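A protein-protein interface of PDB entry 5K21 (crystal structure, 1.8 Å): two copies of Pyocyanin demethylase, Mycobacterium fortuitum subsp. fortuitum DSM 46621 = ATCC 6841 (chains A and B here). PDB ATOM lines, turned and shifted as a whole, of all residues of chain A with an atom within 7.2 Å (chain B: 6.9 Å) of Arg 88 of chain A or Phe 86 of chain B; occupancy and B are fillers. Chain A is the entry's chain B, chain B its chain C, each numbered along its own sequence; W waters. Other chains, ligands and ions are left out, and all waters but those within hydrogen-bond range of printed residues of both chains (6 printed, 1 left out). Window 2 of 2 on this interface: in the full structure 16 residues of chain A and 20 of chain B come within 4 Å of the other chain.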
ATOM      1  N   TYR A  73       8.846 -14.865  32.344  1.00  0.00           N
ATOM      2  CA  TYR A  73       9.156 -14.465  30.987  1.00  0.00           C
ATOM      3  C   TYR A  73      10.194 -15.444  30.453  1.00  0.00           C
ATOM      4  O   TYR A  73      11.279 -15.570  31.032  1.00  0.00           O
ATOM      5  CB  TYR A  73       9.669 -13.028  30.966  1.00  0.00           C
ATOM      6  CG  TYR A  73      10.371 -12.668  29.692  1.00  0.00           C
ATOM      7  CD1 TYR A  73       9.770 -12.898  28.466  1.00  0.00           C
ATOM      8  CD2 TYR A  73      11.631 -12.090  29.707  1.00  0.00           C
ATOM      9  CE1 TYR A  73      10.410 -12.586  27.288  1.00  0.00           C
ATOM     10  CE2 TYR A  73      12.279 -11.766  28.526  1.00  0.00           C
ATOM     11  CZ  TYR A  73      11.656 -12.011  27.324  1.00  0.00           C
ATOM     12  OH  TYR A  73      12.281 -11.696  26.138  1.00  0.00           O
ATOM     13  N   CYS A  74       9.843 -16.177  29.394  1.00  0.00           N
ATOM     14  CA  CYS A  74      10.726 -17.191  28.826  1.00  0.00           C
ATOM     15  C   CYS A  74      11.037 -16.880  27.372  1.00  0.00           C
ATOM     16  O   CYS A  74      10.178 -16.392  26.618  1.00  0.00           O
ATOM     17  CB  CYS A  74      10.118 -18.582  28.894  1.00  0.00           C
ATOM     18  SG  CYS A  74       9.875 -19.198  30.541  1.00  0.00           S
ATOM     19  N   GLU A  75      12.284 -17.148  27.012  1.00  0.00           N
ATOM     20  CA  GLU A  75      12.785 -17.068  25.649  1.00  0.00           C
ATOM     21  C   GLU A  75      13.393 -18.414  25.290  1.00  0.00           C
ATOM     22  O   GLU A  75      14.147 -18.993  26.082  1.00  0.00           O
ATOM     23  CB  GLU A  75      13.856 -15.976  25.495  1.00  0.00           C
ATOM     24  CG  GLU A  75      13.354 -14.551  25.378  1.00  0.00           C
ATOM     25  CD  GLU A  75      12.899 -14.192  23.960  1.00  0.00           C
ATOM     26  OE1 GLU A  75      12.888 -15.083  23.070  1.00  0.00           O
ATOM     27  OE2 GLU A  75      12.582 -13.006  23.731  1.00  0.00           O
ATOM     28  N   LEU A  76      13.089 -18.887  24.082  1.00  0.00           N
ATOM     29  CA  LEU A  76      13.492 -20.207  23.637  1.00  0.00           C
ATOM     30  C   LEU A  76      13.969 -20.125  22.199  1.00  0.00           C
ATOM     31  O   LEU A  76      13.344 -19.453  21.376  1.00  0.00           O
ATOM     32  CB  LEU A  76      12.309 -21.192  23.733  1.00  0.00           C
ATOM     33  CG  LEU A  76      12.531 -22.641  23.302  1.00  0.00           C
ATOM     34  CD1 LEU A  76      13.465 -23.332  24.298  1.00  0.00           C
ATOM     35  CD2 LEU A  76      11.190 -23.354  23.236  1.00  0.00           C
ATOM     36  N   PHE A  86      12.208 -19.387  16.974  1.00  0.00           N
ATOM     37  CA  PHE A  86      12.271 -18.514  18.142  1.00  0.00           C
ATOM     38  C   PHE A  86      10.897 -18.398  18.776  1.00  0.00           C
ATOM     39  O   PHE A  86       9.907 -18.193  18.079  1.00  0.00           O
ATOM     40  CB  PHE A  86      12.747 -17.119  17.757  1.00  0.00           C
ATOM     41  CG  PHE A  86      13.984 -17.121  16.926  1.00  0.00           C
ATOM     42  CD1 PHE A  86      15.042 -17.933  17.250  1.00  0.00           C
ATOM     43  CD2 PHE A  86      14.071 -16.312  15.809  1.00  0.00           C
ATOM     44  CE1 PHE A  86      16.181 -17.947  16.476  1.00  0.00           C
ATOM     45  CE2 PHE A  86      15.191 -16.319  15.022  1.00  0.00           C
ATOM     46  CZ  PHE A  86      16.253 -17.123  15.352  1.00  0.00           C
ATOM     47  N   ALA A  87      10.842 -18.508  20.101  1.00  0.00           N
ATOM     48  CA  ALA A  87       9.584 -18.430  20.816  1.00  0.00           C
ATOM     49  C   ALA A  87       9.773 -17.674  22.121  1.00  0.00           C
ATOM     50  O   ALA A  87      10.868 -17.632  22.692  1.00  0.00           O
ATOM     51  CB  ALA A  87       9.028 -19.823  21.106  1.00  0.00           C
ATOM     52  N   ARG A  88       8.677 -17.102  22.610  1.00  0.00           N
ATOM     53  CA  ARG A  88       8.716 -16.389  23.880  1.00  0.00           C
ATOM     54  C   ARG A  88       7.353 -16.487  24.545  1.00  0.00           C
ATOM     55  O   ARG A  88       6.329 -16.674  23.885  1.00  0.00           O
ATOM     56  CB  ARG A  88       9.114 -14.922  23.704  1.00  0.00           C
ATOM     57  CG  ARG A  88       8.097 -14.111  22.914  1.00  0.00           C
ATOM     58  CD  ARG A  88       8.635 -12.726  22.630  1.00  0.00           C
ATOM     59  NE  ARG A  88       8.600 -11.852  23.802  1.00  0.00           N
ATOM     60  CZ  ARG A  88       9.363 -10.779  23.949  1.00  0.00           C
ATOM     61  NH1 ARG A  88      10.257 -10.467  23.014  1.00  0.00           N
ATOM     62  NH2 ARG A  88       9.253 -10.018  25.031  1.00  0.00           N
ATOM     63  N   SER A  89       7.353 -16.364  25.869  1.00  0.00           N
ATOM     64  CA  SER A  89       6.128 -16.469  26.637  1.00  0.00           C
ATOM     65  C   SER A  89       6.225 -15.590  27.876  1.00  0.00           C
ATOM     66  O   SER A  89       7.319 -15.262  28.353  1.00  0.00           O
ATOM     67  CB  SER A  89       5.815 -17.910  27.050  1.00  0.00           C
ATOM     68  OG  SER A  89       6.884 -18.503  27.777  1.00  0.00           O
ATOM     69  N   LEU A  90       5.053 -15.179  28.358  1.00  0.00           N
ATOM     70  CA  LEU A  90       4.894 -14.604  29.691  1.00  0.00           C
ATOM     71  C   LEU A  90       3.693 -15.327  30.291  1.00  0.00           C
ATOM     72  O   LEU A  90       2.542 -14.989  29.989  1.00  0.00           O
ATOM     73  CB  LEU A  90       4.686 -13.097  29.641  1.00  0.00           C
ATOM     74  CG  LEU A  90       4.450 -12.442  31.009  1.00  0.00           C
ATOM     75  CD1 LEU A  90       5.735 -12.485  31.831  1.00  0.00           C
ATOM     76  CD2 LEU A  90       3.977 -11.007  30.874  1.00  0.00           C
ATOM     77  N   THR A  91       3.945 -16.358  31.082  1.00  0.00           N
ATOM     78  CA  THR A  91       2.864 -17.244  31.514  1.00  0.00           C
ATOM     79  C   THR A  91       3.190 -17.731  32.899  1.00  0.00           C
ATOM     80  O   THR A  91       4.339 -17.650  33.351  1.00  0.00           O
ATOM     81  CB  THR A  91       2.715 -18.457  30.584  1.00  0.00           C
ATOM     82  OG1 THR A  91       3.903 -19.254  30.677  1.00  0.00           O
ATOM     83  CG2 THR A  91       2.520 -18.054  29.136  1.00  0.00           C
ATOM     84  N   THR A  99       1.448 -21.912  26.420  1.00  0.00           N
ATOM     85  CA  THR A  99       1.629 -21.639  25.006  1.00  0.00           C
ATOM     86  C   THR A  99       2.508 -20.413  24.842  1.00  0.00           C
ATOM     87  O   THR A  99       2.247 -19.358  25.430  1.00  0.00           O
ATOM     88  CB  THR A  99       0.287 -21.454  24.313  1.00  0.00           C
ATOM     89  OG1 THR A  99      -0.443 -22.684  24.389  1.00  0.00           O
ATOM     90  CG2 THR A  99       0.486 -21.069  22.839  1.00  0.00           C
ATOM     91  N   MET A 100       3.547 -20.572  24.050  1.00  0.00           N
ATOM     92  CA  MET A 100       4.502 -19.540  23.691  1.00  0.00           C
ATOM     93  C   MET A 100       4.161 -19.015  22.312  1.00  0.00           C
ATOM     94  O   MET A 100       3.542 -19.710  21.498  1.00  0.00           O
ATOM     95  CB  MET A 100       5.937 -20.088  23.679  1.00  0.00           C
ATOM     96  CG  MET A 100       6.322 -20.907  24.894  1.00  0.00           C
ATOM     97  SD  MET A 100       8.062 -21.399  24.836  1.00  0.00           S
ATOM     98  CE  MET A 100       8.859 -19.834  25.181  1.00  0.00           C
ATOM     99  N   ALA A 101       4.521 -17.766  22.073  1.00  0.00           N
ATOM    100  CA  ALA A 101       4.386 -17.172  20.760  1.00  0.00           C
ATOM    101  C   ALA A 101       5.639 -17.492  19.966  1.00  0.00           C
ATOM    102  O   ALA A 101       6.752 -17.290  20.455  1.00  0.00           O
ATOM    103  CB  ALA A 101       4.180 -15.660  20.858  1.00  0.00           C
ATOM    104  N   ILE A 102       5.459 -18.019  18.756  1.00  0.00           N
ATOM    105  CA  ILE A 102       6.582 -18.149  17.839  1.00  0.00           C
ATOM    106  C   ILE A 102       6.741 -16.815  17.133  1.00  0.00           C
ATOM    107  O   ILE A 102       5.817 -16.357  16.452  1.00  0.00           O
ATOM    108  CB  ILE A 102       6.356 -19.283  16.830  1.00  0.00           C
ATOM    109  CG1 ILE A 102       6.439 -20.635  17.538  1.00  0.00           C
ATOM    110  CG2 ILE A 102       7.393 -19.201  15.709  1.00  0.00           C
ATOM    111  CD1 ILE A 102       6.056 -21.808  16.639  1.00  0.00           C
ATOM    112  N   THR A 103       7.916 -16.191  17.294  1.00  0.00           N
ATOM    113  CA  THR A 103       8.134 -14.846  16.776  1.00  0.00           C
ATOM    114  C   THR A 103       8.935 -14.807  15.488  1.00  0.00           C
ATOM    115  O   THR A 103       8.964 -13.761  14.832  1.00  0.00           O
ATOM    116  CB  THR A 103       8.857 -13.977  17.803  1.00  0.00           C
ATOM    117  OG1 THR A 103      10.107 -14.589  18.101  1.00  0.00           O
ATOM    118  CG2 THR A 103       8.035 -13.828  19.076  1.00  0.00           C
ATOM    119  N   LYS A 113       5.577 -17.301  12.036  1.00  0.00           N
ATOM    120  CA  LYS A 113       4.855 -16.898  13.231  1.00  0.00           C
ATOM    121  C   LYS A 113       4.052 -18.099  13.692  1.00  0.00           C
ATOM    122  O   LYS A 113       3.941 -19.107  12.984  1.00  0.00           O
ATOM    123  CB  LYS A 113       3.917 -15.705  12.991  1.00  0.00           C
ATOM    124  CG  LYS A 113       4.595 -14.429  12.543  1.00  0.00           C
ATOM    125  CD  LYS A 113       5.414 -13.849  13.684  1.00  0.00           C
ATOM    126  CE  LYS A 113       6.040 -12.512  13.318  1.00  0.00           C
ATOM    127  NZ  LYS A 113       6.885 -11.990  14.448  1.00  0.00           N
ATOM    128  N   LEU A 116       3.538 -22.261  20.177  1.00  0.00           N
ATOM    129  CA  LEU A 116       4.206 -23.473  20.618  1.00  0.00           C
ATOM    130  C   LEU A 116       3.708 -23.788  22.017  1.00  0.00           C
ATOM    131  O   LEU A 116       3.898 -22.986  22.937  1.00  0.00           O
ATOM    132  CB  LEU A 116       5.718 -23.265  20.566  1.00  0.00           C
ATOM    133  CG  LEU A 116       6.681 -24.404  20.908  1.00  0.00           C
ATOM    134  CD1 LEU A 116       8.048 -24.059  20.394  1.00  0.00           C
ATOM    135  CD2 LEU A 116       6.788 -24.622  22.404  1.00  0.00           C
ATOM    136  N   GLY B  57       5.740  -8.132  32.288  1.00  0.00           N
ATOM    137  CA  GLY B  57       6.903  -8.731  32.909  1.00  0.00           C
ATOM    138  C   GLY B  57       8.104  -8.434  32.047  1.00  0.00           C
ATOM    139  O   GLY B  57       7.976  -8.402  30.822  1.00  0.00           O
ATOM    140  N   GLU B  75      13.945  -6.129  27.833  1.00  0.00           N
ATOM    141  CA  GLU B  75      12.937  -6.918  27.156  1.00  0.00           C
ATOM    142  C   GLU B  75      11.676  -6.814  27.998  1.00  0.00           C
ATOM    143  O   GLU B  75      11.737  -6.928  29.223  1.00  0.00           O
ATOM    144  CB  GLU B  75      13.385  -8.385  27.031  1.00  0.00           C
ATOM    145  CG  GLU B  75      14.409  -8.648  25.954  1.00  0.00           C
ATOM    146  CD  GLU B  75      13.794  -8.753  24.557  1.00  0.00           C
ATOM    147  OE1 GLU B  75      12.565  -8.533  24.410  1.00  0.00           O
ATOM    148  OE2 GLU B  75      14.543  -9.064  23.605  1.00  0.00           O
ATOM    149  N   LEU B  76      10.536  -6.596  27.347  1.00  0.00           N
ATOM    150  CA  LEU B  76       9.280  -6.404  28.048  1.00  0.00           C
ATOM    151  C   LEU B  76       8.170  -7.141  27.313  1.00  0.00           C
ATOM    152  O   LEU B  76       8.142  -7.157  26.080  1.00  0.00           O
ATOM    153  CB  LEU B  76       8.920  -4.914  28.153  1.00  0.00           C
ATOM    154  CG  LEU B  76       7.616  -4.591  28.889  1.00  0.00           C
ATOM    155  CD1 LEU B  76       7.758  -4.799  30.400  1.00  0.00           C
ATOM    156  CD2 LEU B  76       7.174  -3.179  28.534  1.00  0.00           C
ATOM    157  N   THR B  77       7.276  -7.771  28.069  1.00  0.00           N
ATOM    158  CA  THR B  77       6.041  -8.321  27.523  1.00  0.00           C
ATOM    159  C   THR B  77       4.870  -7.721  28.280  1.00  0.00           C
ATOM    160  O   THR B  77       4.825  -7.795  29.511  1.00  0.00           O
ATOM    161  CB  THR B  77       6.000  -9.839  27.637  1.00  0.00           C
ATOM    162  OG1 THR B  77       7.102 -10.400  26.920  1.00  0.00           O
ATOM    163  CG2 THR B  77       4.689 -10.388  27.068  1.00  0.00           C
ATOM    164  N   ILE B  78       3.940  -7.134  27.532  1.00  0.00           N
ATOM    165  CA  ILE B  78       2.692  -6.586  28.051  1.00  0.00           C
ATOM    166  C   ILE B  78       1.585  -7.582  27.740  1.00  0.00           C
ATOM    167  O   ILE B  78       1.515  -8.107  26.622  1.00  0.00           O
ATOM    168  CB  ILE B  78       2.400  -5.211  27.429  1.00  0.00           C
ATOM    169  CG1 ILE B  78       3.367  -4.175  28.013  1.00  0.00           C
ATOM    170  CG2 ILE B  78       0.955  -4.755  27.714  1.00  0.00           C
ATOM    171  CD1 ILE B  78       3.374  -2.864  27.277  1.00  0.00           C
ATOM    172  N   GLU B  84      -0.970 -10.044  23.693  1.00  0.00           N
ATOM    173  CA  GLU B  84       0.286  -9.593  24.260  1.00  0.00           C
ATOM    174  C   GLU B  84       1.015  -8.696  23.266  1.00  0.00           C
ATOM    175  O   GLU B  84       0.722  -8.680  22.067  1.00  0.00           O
ATOM    176  CB  GLU B  84       1.157 -10.787  24.674  1.00  0.00           C
ATOM    177  CG  GLU B  84       0.571 -11.548  25.867  1.00  0.00           C
ATOM    178  CD  GLU B  84       1.473 -12.646  26.404  1.00  0.00           C
ATOM    179  OE1 GLU B  84       2.248 -13.220  25.615  1.00  0.00           O
ATOM    180  OE2 GLU B  84       1.396 -12.941  27.622  1.00  0.00           O
ATOM    181  N   ILE B  85       1.933  -7.902  23.800  1.00  0.00           N
ATOM    182  CA  ILE B  85       2.762  -6.984  23.031  1.00  0.00           C
ATOM    183  C   ILE B  85       4.208  -7.166  23.492  1.00  0.00           C
ATOM    184  O   ILE B  85       4.473  -7.200  24.697  1.00  0.00           O
ATOM    185  CB  ILE B  85       2.299  -5.528  23.231  1.00  0.00           C
ATOM    186  CG1 ILE B  85       0.844  -5.371  22.782  1.00  0.00           C
ATOM    187  CG2 ILE B  85       3.208  -4.564  22.490  1.00  0.00           C
ATOM    188  CD1 ILE B  85       0.231  -4.039  23.136  1.00  0.00           C
ATOM    189  N   PHE B  86       5.131  -7.298  22.540  1.00  0.00           N
ATOM    190  CA  PHE B  86       6.540  -7.544  22.842  1.00  0.00           C
ATOM    191  C   PHE B  86       7.368  -6.306  22.511  1.00  0.00           C
ATOM    192  O   PHE B  86       7.225  -5.734  21.434  1.00  0.00           O
ATOM    193  CB  PHE B  86       7.067  -8.740  22.042  1.00  0.00           C
ATOM    194  CG  PHE B  86       6.197  -9.969  22.119  1.00  0.00           C
ATOM    195  CD1 PHE B  86       5.654 -10.390  23.327  1.00  0.00           C
ATOM    196  CD2 PHE B  86       5.942 -10.721  20.973  1.00  0.00           C
ATOM    197  CE1 PHE B  86       4.865 -11.532  23.388  1.00  0.00           C
ATOM    198  CE2 PHE B  86       5.151 -11.857  21.034  1.00  0.00           C
ATOM    199  CZ  PHE B  86       4.621 -12.268  22.239  1.00  0.00           C
ATOM    200  N   ALA B  87       8.241  -5.899  23.423  1.00  0.00           N
ATOM    201  CA  ALA B  87       9.080  -4.739  23.173  1.00  0.00           C
ATOM    202  C   ALA B  87      10.494  -4.978  23.696  1.00  0.00           C
ATOM    203  O   ALA B  87      10.729  -5.786  24.607  1.00  0.00           O
ATOM    204  CB  ALA B  87       8.507  -3.486  23.814  1.00  0.00           C
ATOM    205  N   ARG B  88      11.435  -4.236  23.115  1.00  0.00           N
ATOM    206  CA  ARG B  88      12.842  -4.322  23.494  1.00  0.00           C
ATOM    207  C   ARG B  88      13.517  -2.977  23.276  1.00  0.00           C
ATOM    208  O   ARG B  88      13.102  -2.185  22.426  1.00  0.00           O
ATOM    209  CB  ARG B  88      13.573  -5.408  22.701  1.00  0.00           C
ATOM    210  CG  ARG B  88      13.624  -5.175  21.202  1.00  0.00           C
ATOM    211  CD  ARG B  88      14.270  -6.385  20.540  1.00  0.00           C
ATOM    212  NE  ARG B  88      15.723  -6.413  20.687  1.00  0.00           N
ATOM    213  CZ  ARG B  88      16.460  -7.527  20.602  1.00  0.00           C
ATOM    214  NH1 ARG B  88      15.880  -8.708  20.422  1.00  0.00           N
ATOM    215  NH2 ARG B  88      17.777  -7.473  20.725  1.00  0.00           N
ATOM    216  N   ALA B 101      11.252  -0.569  21.078  1.00  0.00           N
ATOM    217  CA  ALA B 101      10.688  -1.021  19.824  1.00  0.00           C
ATOM    218  C   ALA B 101       9.680  -2.118  20.116  1.00  0.00           C
ATOM    219  O   ALA B 101       9.995  -3.082  20.819  1.00  0.00           O
ATOM    220  CB  ALA B 101      11.791  -1.542  18.908  1.00  0.00           C
ATOM    221  N   ILE B 102       8.472  -1.972  19.583  1.00  0.00           N
ATOM    222  CA  ILE B 102       7.505  -3.057  19.637  1.00  0.00           C
ATOM    223  C   ILE B 102       7.790  -3.971  18.457  1.00  0.00           C
ATOM    224  O   ILE B 102       7.728  -3.555  17.296  1.00  0.00           O
ATOM    225  CB  ILE B 102       6.061  -2.531  19.640  1.00  0.00           C
ATOM    226  CG1 ILE B 102       5.773  -1.886  20.999  1.00  0.00           C
ATOM    227  CG2 ILE B 102       5.058  -3.654  19.346  1.00  0.00           C
ATOM    228  CD1 ILE B 102       4.437  -1.263  21.146  1.00  0.00           C
ATOM    229  N   THR B 103       8.131  -5.218  18.757  1.00  0.00           N
ATOM    230  CA  THR B 103       8.570  -6.162  17.740  1.00  0.00           C
ATOM    231  C   THR B 103       7.468  -7.112  17.306  1.00  0.00           C
ATOM    232  O   THR B 103       7.601  -7.755  16.264  1.00  0.00           O
ATOM    233  CB  THR B 103       9.745  -6.975  18.279  1.00  0.00           C
ATOM    234  OG1 THR B 103       9.317  -7.657  19.463  1.00  0.00           O
ATOM    235  CG2 THR B 103      10.918  -6.062  18.625  1.00  0.00           C
ATOM    236  N   GLY B 104       6.384  -7.203  18.064  1.00  0.00           N
ATOM    237  CA  GLY B 104       5.307  -8.096  17.703  1.00  0.00           C
ATOM    238  C   GLY B 104       4.352  -8.241  18.867  1.00  0.00           C
ATOM    239  O   GLY B 104       4.434  -7.517  19.861  1.00  0.00           O
ATOM    240  N   GLY B 105       3.466  -9.214  18.732  1.00  0.00           N
ATOM    241  CA  GLY B 105       2.477  -9.463  19.756  1.00  0.00           C
ATOM    242  C   GLY B 105       1.644 -10.662  19.378  1.00  0.00           C
ATOM    243  O   GLY B 105       1.976 -11.399  18.444  1.00  0.00           O
ATOM    244  N   THR B 106       0.570 -10.864  20.137  1.00  0.00           N
ATOM    245  CA  THR B 106      -0.355 -11.965  19.907  1.00  0.00           C
ATOM    246  C   THR B 106      -1.771 -11.419  19.873  1.00  0.00           C
ATOM    247  O   THR B 106      -2.023 -10.265  20.240  1.00  0.00           O
ATOM    248  CB  THR B 106      -0.237 -13.045  20.989  1.00  0.00           C
ATOM    249  OG1 THR B 106      -0.620 -12.503  22.261  1.00  0.00           O
ATOM    250  CG2 THR B 106       1.197 -13.581  21.072  1.00  0.00           C
ATOM    251  N   TYR B 109      -2.877  -8.076  18.541  1.00  0.00           N
ATOM    252  CA  TYR B 109      -1.610  -7.410  18.268  1.00  0.00           C
ATOM    253  C   TYR B 109      -0.626  -8.297  17.514  1.00  0.00           C
ATOM    254  O   TYR B 109       0.559  -7.963  17.439  1.00  0.00           O
ATOM    255  CB  TYR B 109      -0.983  -6.914  19.581  1.00  0.00           C
ATOM    256  CG  TYR B 109      -2.001  -6.225  20.457  1.00  0.00           C
ATOM    257  CD1 TYR B 109      -2.578  -5.027  20.059  1.00  0.00           C
ATOM    258  CD2 TYR B 109      -2.408  -6.783  21.666  1.00  0.00           C
ATOM    259  CE1 TYR B 109      -3.544  -4.397  20.830  1.00  0.00           C
ATOM    260  CE2 TYR B 109      -3.370  -6.155  22.457  1.00  0.00           C
ATOM    261  CZ  TYR B 109      -3.931  -4.958  22.029  1.00  0.00           C
ATOM    262  OH  TYR B 109      -4.888  -4.309  22.785  1.00  0.00           O
ATOM    263  N   SER B 112       2.024  -6.899  14.877  1.00  0.00           N
ATOM    264  CA  SER B 112       2.088  -5.476  15.152  1.00  0.00           C
ATOM    265  C   SER B 112       3.539  -5.028  15.253  1.00  0.00           C
ATOM    266  O   SER B 112       4.431  -5.797  15.623  1.00  0.00           O
ATOM    267  CB  SER B 112       1.330  -5.114  16.436  1.00  0.00           C
ATOM    268  OG  SER B 112       1.981  -5.607  17.588  1.00  0.00           O
ATOM    269  N   GLY B 114       5.687  -1.005  16.198  1.00  0.00           N
ATOM    270  CA  GLY B 114       5.489   0.326  16.739  1.00  0.00           C
ATOM    271  C   GLY B 114       6.447   0.638  17.867  1.00  0.00           C
ATOM    272  O   GLY B 114       7.545   0.071  17.951  1.00  0.00           O
ATOM    273  N   LEU B 116       6.997   1.973  22.173  1.00  0.00           N
ATOM    274  CA  LEU B 116       6.529   2.063  23.550  1.00  0.00           C
ATOM    275  C   LEU B 116       7.503   2.963  24.275  1.00  0.00           C
ATOM    276  O   LEU B 116       8.666   2.594  24.458  1.00  0.00           O
ATOM    277  CB  LEU B 116       6.493   0.687  24.225  1.00  0.00           C
ATOM    278  CG  LEU B 116       5.911   0.547  25.634  1.00  0.00           C
ATOM    279  CD1 LEU B 116       5.699  -0.912  25.936  1.00  0.00           C
ATOM    280  CD2 LEU B 116       6.802   1.121  26.692  1.00  0.00           C
HETATM  281  O   HOH W   1       2.884 -16.401  24.654  1.00  0.00           O
HETATM  282  O   HOH W   2       6.925 -13.109  26.149  1.00  0.00           O
HETATM  283  O   HOH W   3       2.696 -15.675  26.987  1.00  0.00           O
HETATM  284  O   HOH W   4      11.230  -8.051  21.267  1.00  0.00           O
HETATM  285  O   HOH W   5      13.739 -11.251  21.465  1.00  0.00           O
HETATM  286  O   HOH W   6       4.672 -14.341  25.088  1.00  0.00           O
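NH1 of Arg 88 of chain A is in salt-bridge range of OE1 of Glu 75 of chain B.
The guanidinium group (NH2) of Arg 88 of chain A lies within hydrogen-bond range of the backbone carbonyl oxygen (O) of Leu 76 of chain B (3.2 Å).
The guanidinium group (NH2) of Arg 88 of chain A sits at hydrogen-bond distance from the side-chain hydroxyl (OG1) of Thr 77 of chain B (2.9 Å).
O of Leu 90 of chain A sits close to OE2 of Glu 84 of chain B.
The backbone carbonyl oxygen (O) of Arg 88 of chain A lies within hydrogen-bond range of the backbone NH (N) of Ala 101 of chain A.
The backbone carbonyl oxygen (O) of Gly 57 of chain B sits at hydrogen-bond distance from the backbone NH (N) of Thr 77 of chain B (2.9 Å).
NH1 of Arg 88 of chain B is in salt-bridge range of OE2 of Glu 75 of chain B (3.5 Å).
The backbone carbonyl oxygen (O) of Ala 87 of chain B sits at hydrogen-bond distance from the backbone NH (N) of Leu 76 of chain B, 2.9 Å away.
The side-chain hydroxyl (OG1) of Thr 106 of chain B is in hydrogen-bond range of the backbone NH (N) of Glu 84 of chain B, at 2.9 Å.
N of Thr 103 of chain B lies within hydrogen-bond range of O of Phe 86 of chain B, at 2.9 Å.
Among the printed residues, pairs that only touch across the chains: Arg 88 of chain A with Phe 86 of chain B (3.3 Å), Leu 90 of chain A with Thr 77 of chain B (3.6 Å), Tyr 73 of chain A with Glu 75 of chain B (3.6 Å), Ala 101 of chain A with Thr 106 of chain B (3.6 Å), Leu 90 of chain A with Gly 57 of chain B (3.7 Å), Ala 101 of chain A with Phe 86 of chain B (3.7 Å) and Tyr 73 of chain A with Thr 77 of chain B (3.97 Å).
Of the printed residues of chain B, Tyr 73 of chain A touches Glu 75 (3.6 Å) and Thr 77 (3.97 Å).
Arg 88 of chain A touches just these residues of chain B: Glu 75 (3.3 Å), Leu 76 (3.2 Å), Thr 77 (2.9 Å) and Phe 86 (3.3 Å).
Printed residues of chain A within 4 Å of Gly 57 of chain B: Leu 90.
Of the printed residues of chain A, Leu 76 of chain B touches Arg 88 (3.2 Å).
Of the printed residues of chain A, Thr 77 of chain B touches Tyr 73, Arg 88 and Leu 90.
Ile 85 of chain B touches none of the printed residues of chain A.
Of the printed residues of chain A, Phe 86 of chain B touches Arg 88 (3.3 Å) and Ala 101 (3.7 Å).
The nearest residue of chain B that does not touch Arg 88 of chain A is Ala 87 of chain B (4.5 Å).
The nearest printed residue of chain A that does not touch Leu 76 of chain B is Tyr 73 of chain A (5.5 Å).
Hydrophobic or aromatic side chains of chain A that line the printed part of chain B: Tyr 73, Leu 90 and Ala 101.
Of the 20 printed residues of chain B, 7 touch a printed residue of chain A.
Among the printed residues, 11 pairs touch across the chains.
Among the printed residues, Asp or Glu carboxylates within 4 Å of a Lys or Arg side-chain nitrogen of the other chain: Arg 88 of chain A with Glu 75 of chain B.
Arg 88 of chain A touches Glu 75 of chain B, but with the chains exchanged Glu 75 of chain A does not touch Arg 88 of chain B (6.3 Å).
Arg 88 of chain A touches Leu 76 of chain B, but with the chains exchanged Leu 76 of chain A does not touch Arg 88 of chain B (11.1 Å).
Arg 88 of chain A touches Phe 86 of chain B, but with the chains exchanged Phe 86 of chain A does not touch Arg 88 of chain B (9.1 Å).
Ala 101 of chain A touches Phe 86 of chain B, but with the chains exchanged Phe 86 of chain A does not touch Ala 101 of chain B (14.6 Å).
Of the 11 pairs that touch across the chains among the printed residues, none has its exchanged pair printed and touching as well.
Water W4 lies within hydrogen-bond range of the side-chain hydroxyl of Thr 103 of chain B, the guanidinium group of Arg 88 of chain A and the side-chain carboxylate of Glu 75 of chain B.
Water W6 lies within hydrogen-bond range of OE1 of Glu 84 of chain B (2.7 Å), O of Arg 88 of chain A (3.1 Å), N of Leu 90 of chain A (3.4 Å) and N of Ser 89 of chain A (3.4 Å).
Water W3 lies within hydrogen-bond range of the backbone NH of Leu 90 of chain A and the side-chain carboxylate of Glu 84 of chain B.
Water W2 lies within hydrogen-bond range of OG1 of Thr 77 of chain B (2.8 Å), O of Ser 89 of chain A (3.1 Å) and NE of Arg 88 of chain A (3.1 Å).
Water W5 lies within hydrogen-bond range of OE2 of Glu 75 of chain A (3.1 Å), OE2 of Glu 75 of chain B (3.2 Å) and NH1 of Arg 88 of chain B (3.5 Å).
Water W1 lies within hydrogen-bond range of O of Thr 99 of chain A (3.1 Å), N of Ala 101 of chain A (3.3 Å) and OE1 of Glu 84 of chain B (3.4 Å).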
